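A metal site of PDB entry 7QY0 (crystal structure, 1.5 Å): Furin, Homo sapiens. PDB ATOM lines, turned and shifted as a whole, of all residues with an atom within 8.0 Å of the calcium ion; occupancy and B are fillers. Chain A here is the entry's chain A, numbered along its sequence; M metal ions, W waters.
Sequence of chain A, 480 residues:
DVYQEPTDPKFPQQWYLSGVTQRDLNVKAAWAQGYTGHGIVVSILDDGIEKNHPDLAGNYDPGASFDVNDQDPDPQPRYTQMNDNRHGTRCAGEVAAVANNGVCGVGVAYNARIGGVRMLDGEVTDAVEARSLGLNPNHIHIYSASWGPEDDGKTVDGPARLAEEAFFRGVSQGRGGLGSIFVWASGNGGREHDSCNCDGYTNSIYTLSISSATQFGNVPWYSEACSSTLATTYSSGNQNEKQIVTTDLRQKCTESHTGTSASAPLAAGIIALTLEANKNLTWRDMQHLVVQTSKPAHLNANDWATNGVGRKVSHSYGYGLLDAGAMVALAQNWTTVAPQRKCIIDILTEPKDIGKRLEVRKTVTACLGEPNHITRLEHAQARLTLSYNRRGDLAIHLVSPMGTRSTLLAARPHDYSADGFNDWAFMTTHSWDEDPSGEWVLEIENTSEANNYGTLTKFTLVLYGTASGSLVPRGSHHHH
Within 4 Å of the calcium ion: Asp 67, Asp 72 and Asp 74.
OD2 of Asp 67 binds the calcium ion (2.3 Å).
Water W2 is bound to the calcium ion, at 2.4 Å.
Water W3 binds the calcium ion.
The calcium ion is bound by OD1 of Asp 72, at 2.4 Å.
The backbone carbonyl oxygen (O) of Asp 74 is bound to the calcium ion, at 2.5 Å.
Water W1 is bound to the calcium ion (2.5 Å).
OD2 of Asp 72 binds the calcium ion, 2.5 Å away.
OD1 of Asp 67 lies within hydrogen-bond range of N of Asn 69, at 3.1 Å.
The side-chain amino group of Lys 51 lies within salt-bridge range of the side-chain carboxylate of Asp 74.
N of Gln 76 lies within hydrogen-bond range of OD1 of Asp 74.
OD1 of Asp 67 sits at hydrogen-bond distance from N of Asp 70, 2.9 Å away.
The side-chain carboxylate of Asp 67 is in salt-bridge range of the guanidinium group of Arg 118 (3.3 Å).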
ATOM      1  N   LYS A  51     -31.783 -29.703 -30.325  1.00  0.00           N
ATOM      2  CA  LYS A  51     -31.430 -28.764 -31.381  1.00  0.00           C
ATOM      3  C   LYS A  51     -31.586 -29.370 -32.760  1.00  0.00           C
ATOM      4  O   LYS A  51     -31.712 -28.627 -33.743  1.00  0.00           O
ATOM      5  CB  LYS A  51     -30.010 -28.262 -31.151  1.00  0.00           C
ATOM      6  CG  LYS A  51     -28.904 -29.268 -31.341  1.00  0.00           C
ATOM      7  CD  LYS A  51     -27.598 -28.740 -30.766  1.00  0.00           C
ATOM      8  CE  LYS A  51     -26.489 -29.755 -30.846  1.00  0.00           C
ATOM      9  NZ  LYS A  51     -26.674 -30.855 -29.851  1.00  0.00           N
ATOM     10  N   PHE A  66     -26.416 -22.750 -24.095  1.00  0.00           N
ATOM     11  CA  PHE A  66     -25.317 -23.223 -23.254  1.00  0.00           C
ATOM     12  C   PHE A  66     -25.843 -24.311 -22.322  1.00  0.00           C
ATOM     13  O   PHE A  66     -27.047 -24.455 -22.125  1.00  0.00           O
ATOM     14  CB  PHE A  66     -24.682 -22.067 -22.462  1.00  0.00           C
ATOM     15  CG  PHE A  66     -23.250 -22.296 -22.123  1.00  0.00           C
ATOM     16  CD1 PHE A  66     -22.256 -22.038 -23.053  1.00  0.00           C
ATOM     17  CD2 PHE A  66     -22.887 -22.762 -20.871  1.00  0.00           C
ATOM     18  CE1 PHE A  66     -20.922 -22.261 -22.741  1.00  0.00           C
ATOM     19  CE2 PHE A  66     -21.565 -22.972 -20.558  1.00  0.00           C
ATOM     20  CZ  PHE A  66     -20.590 -22.725 -21.486  1.00  0.00           C
ATOM     21  N   ASP A  67     -24.923 -25.098 -21.777  1.00  0.00           N
ATOM     22  CA  ASP A  67     -25.242 -26.160 -20.835  1.00  0.00           C
ATOM     23  C   ASP A  67     -24.518 -25.797 -19.544  1.00  0.00           C
ATOM     24  O   ASP A  67     -23.320 -26.067 -19.395  1.00  0.00           O
ATOM     25  CB  ASP A  67     -24.815 -27.515 -21.390  1.00  0.00           C
ATOM     26  CG  ASP A  67     -25.141 -28.661 -20.464  1.00  0.00           C
ATOM     27  OD1 ASP A  67     -25.489 -28.431 -19.292  1.00  0.00           O
ATOM     28  OD2 ASP A  67     -25.023 -29.825 -20.921  1.00  0.00           O
ATOM     29  N   VAL A  68     -25.243 -25.175 -18.601  1.00  0.00           N
ATOM     30  CA  VAL A  68     -24.637 -24.787 -17.327  1.00  0.00           C
ATOM     31  C   VAL A  68     -24.717 -25.903 -16.290  1.00  0.00           C
ATOM     32  O   VAL A  68     -24.151 -25.758 -15.189  1.00  0.00           O
ATOM     33  CB  VAL A  68     -25.266 -23.514 -16.731  1.00  0.00           C
ATOM     34  CG1 VAL A  68     -25.083 -22.325 -17.677  1.00  0.00           C
ATOM     35  CG2 VAL A  68     -26.742 -23.718 -16.418  1.00  0.00           C
ATOM     36  N   ASN A  69     -25.409 -27.003 -16.587  1.00  0.00           N
ATOM     37  CA  ASN A  69     -25.389 -28.162 -15.693  1.00  0.00           C
ATOM     38  C   ASN A  69     -24.112 -28.978 -15.862  1.00  0.00           C
ATOM     39  O   ASN A  69     -23.522 -29.427 -14.876  1.00  0.00           O
ATOM     40  CB  ASN A  69     -26.621 -29.050 -15.950  1.00  0.00           C
ATOM     41  CG  ASN A  69     -27.942 -28.403 -15.536  1.00  0.00           C
ATOM     42  OD1 ASN A  69     -28.941 -28.476 -16.262  1.00  0.00           O
ATOM     43  ND2 ASN A  69     -27.944 -27.783 -14.357  1.00  0.00           N
ATOM     44  N   ASP A  70     -23.675 -29.198 -17.108  1.00  0.00           N
ATOM     45  CA  ASP A  70     -22.462 -29.960 -17.392  1.00  0.00           C
ATOM     46  C   ASP A  70     -21.313 -29.085 -17.859  1.00  0.00           C
ATOM     47  O   ASP A  70     -20.233 -29.605 -18.161  1.00  0.00           O
ATOM     48  CB  ASP A  70     -22.741 -31.038 -18.460  1.00  0.00           C
ATOM     49  CG  ASP A  70     -23.418 -32.280 -17.897  1.00  0.00           C
ATOM     50  OD1 ASP A  70     -23.315 -32.511 -16.684  1.00  0.00           O
ATOM     51  OD2 ASP A  70     -24.060 -33.023 -18.666  1.00  0.00           O
ATOM     52  N   GLN A  71     -21.506 -27.764 -17.948  1.00  0.00           N
ATOM     53  CA  GLN A  71     -20.452 -26.823 -18.311  1.00  0.00           C
ATOM     54  C   GLN A  71     -19.870 -27.114 -19.702  1.00  0.00           C
ATOM     55  O   GLN A  71     -18.688 -27.400 -19.868  1.00  0.00           O
ATOM     56  CB  GLN A  71     -19.355 -26.821 -17.224  1.00  0.00           C
ATOM     57  CG  GLN A  71     -19.925 -26.606 -15.826  1.00  0.00           C
ATOM     58  CD  GLN A  71     -18.927 -26.050 -14.849  1.00  0.00           C
ATOM     59  N   ASP A  72     -20.728 -27.012 -20.703  1.00  0.00           N
ATOM     60  CA  ASP A  72     -20.327 -27.140 -22.090  1.00  0.00           C
ATOM     61  C   ASP A  72     -21.304 -26.338 -22.935  1.00  0.00           C
ATOM     62  O   ASP A  72     -22.307 -25.830 -22.419  1.00  0.00           O
ATOM     63  CB  ASP A  72     -20.265 -28.611 -22.536  1.00  0.00           C
ATOM     64  CG  ASP A  72     -21.624 -29.310 -22.538  1.00  0.00           C
ATOM     65  OD1 ASP A  72     -22.493 -28.934 -23.347  1.00  0.00           O
ATOM     66  OD2 ASP A  72     -21.814 -30.266 -21.755  1.00  0.00           O
ATOM     67  N   PRO A  73     -21.031 -26.174 -24.232  1.00  0.00           N
ATOM     68  CA  PRO A  73     -21.893 -25.284 -25.033  1.00  0.00           C
ATOM     69  C   PRO A  73     -23.162 -25.934 -25.553  1.00  0.00           C
ATOM     70  O   PRO A  73     -24.011 -25.223 -26.106  1.00  0.00           O
ATOM     71  CB  PRO A  73     -21.009 -24.866 -26.218  1.00  0.00           C
ATOM     72  CG  PRO A  73     -19.667 -25.394 -25.949  1.00  0.00           C
ATOM     73  CD  PRO A  73     -19.798 -26.530 -24.965  1.00  0.00           C
ATOM     74  N   ASP A  74     -23.320 -27.244 -25.392  1.00  0.00           N
ATOM     75  CA  ASP A  74     -24.316 -28.023 -26.105  1.00  0.00           C
ATOM     76  C   ASP A  74     -25.477 -28.342 -25.176  1.00  0.00           C
ATOM     77  O   ASP A  74     -25.308 -29.135 -24.235  1.00  0.00           O
ATOM     78  CB  ASP A  74     -23.655 -29.312 -26.625  1.00  0.00           C
ATOM     79  CG  ASP A  74     -24.595 -30.215 -27.398  1.00  0.00           C
ATOM     80  OD1 ASP A  74     -25.803 -29.947 -27.466  1.00  0.00           O
ATOM     81  OD2 ASP A  74     -24.107 -31.220 -27.940  1.00  0.00           O
ATOM     82  N   PRO A  75     -26.677 -27.764 -25.401  1.00  0.00           N
ATOM     83  CA  PRO A  75     -27.787 -27.940 -24.464  1.00  0.00           C
ATOM     84  C   PRO A  75     -28.679 -29.141 -24.747  1.00  0.00           C
ATOM     85  O   PRO A  75     -29.828 -29.186 -24.301  1.00  0.00           O
ATOM     86  CB  PRO A  75     -28.588 -26.649 -24.645  1.00  0.00           C
ATOM     87  CG  PRO A  75     -28.491 -26.467 -26.183  1.00  0.00           C
ATOM     88  CD  PRO A  75     -27.031 -26.812 -26.484  1.00  0.00           C
ATOM     89  N   GLN A  76     -28.178 -30.103 -25.514  1.00  0.00           N
ATOM     90  CA  GLN A  76     -28.995 -31.261 -25.842  1.00  0.00           C
ATOM     91  C   GLN A  76     -29.511 -31.913 -24.566  1.00  0.00           C
ATOM     92  O   GLN A  76     -28.762 -32.062 -23.582  1.00  0.00           O
ATOM     93  CB  GLN A  76     -28.166 -32.269 -26.642  1.00  0.00           C
ATOM     94  CG  GLN A  76     -29.000 -33.351 -27.340  1.00  0.00           C
ATOM     95  CD  GLN A  76     -29.668 -32.875 -28.621  1.00  0.00           C
ATOM     96  OE1 GLN A  76     -29.366 -31.799 -29.142  1.00  0.00           O
ATOM     97  NE2 GLN A  76     -30.593 -33.678 -29.138  1.00  0.00           N
ATOM     98  N   PRO A  77     -30.791 -32.297 -24.521  1.00  0.00           N
ATOM     99  CA  PRO A  77     -31.336 -32.907 -23.306  1.00  0.00           C
ATOM    100  C   PRO A  77     -30.747 -34.288 -23.032  1.00  0.00           C
ATOM    101  O   PRO A  77     -30.272 -34.992 -23.923  1.00  0.00           O
ATOM    102  CB  PRO A  77     -32.840 -33.006 -23.598  1.00  0.00           C
ATOM    103  CG  PRO A  77     -33.096 -32.112 -24.780  1.00  0.00           C
ATOM    104  CD  PRO A  77     -31.810 -32.087 -25.566  1.00  0.00           C
ATOM    105  N   ARG A  78     -30.818 -34.657 -21.751  1.00  0.00           N
ATOM    106  CA  ARG A  78     -30.507 -36.015 -21.302  1.00  0.00           C
ATOM    107  C   ARG A  78     -31.747 -36.883 -21.515  1.00  0.00           C
ATOM    108  O   ARG A  78     -32.817 -36.605 -20.939  1.00  0.00           O
ATOM    109  CB  ARG A  78     -30.085 -35.963 -19.829  1.00  0.00           C
ATOM    110  CG  ARG A  78     -29.757 -37.302 -19.167  1.00  0.00           C
ATOM    111  CD  ARG A  78     -29.225 -37.086 -17.752  1.00  0.00           C
ATOM    112  NE  ARG A  78     -30.249 -36.411 -16.968  1.00  0.00           N
ATOM    113  CZ  ARG A  78     -31.142 -37.032 -16.217  1.00  0.00           C
ATOM    114  NH1 ARG A  78     -31.134 -38.355 -16.106  1.00  0.00           N
ATOM    115  NH2 ARG A  78     -32.061 -36.332 -15.570  1.00  0.00           N
ATOM    116  N   ARG A 118     -29.483 -25.291 -20.879  1.00  0.00           N
ATOM    117  CA  ARG A 118     -29.704 -26.471 -20.052  1.00  0.00           C
ATOM    118  C   ARG A 118     -29.217 -26.121 -18.655  1.00  0.00           C
ATOM    119  O   ARG A 118     -28.022 -26.071 -18.390  1.00  0.00           O
ATOM    120  CB  ARG A 118     -28.942 -27.659 -20.642  1.00  0.00           C
ATOM    121  CG  ARG A 118     -29.154 -28.980 -19.915  1.00  0.00           C
ATOM    122  CD  ARG A 118     -28.560 -30.189 -20.686  1.00  0.00           C
ATOM    123  NE  ARG A 118     -28.745 -31.368 -19.850  1.00  0.00           N
ATOM    124  CZ  ARG A 118     -27.793 -31.974 -19.145  1.00  0.00           C
ATOM    125  NH1 ARG A 118     -26.529 -31.581 -19.202  1.00  0.00           N
ATOM    126  NH2 ARG A 118     -28.124 -33.005 -18.385  1.00  0.00           N
HETATM  127 CA    CA M   1     -24.062 -30.690 -22.782  1.00  0.00          CA
HETATM  128  O   HOH W   1     -23.753 -32.739 -21.408  1.00  0.00           O
HETATM  129  O   HOH W   2     -25.967 -32.008 -23.410  1.00  0.00           O
HETATM  130  O   HOH W   3     -22.911 -32.027 -24.417  1.00  0.00           O
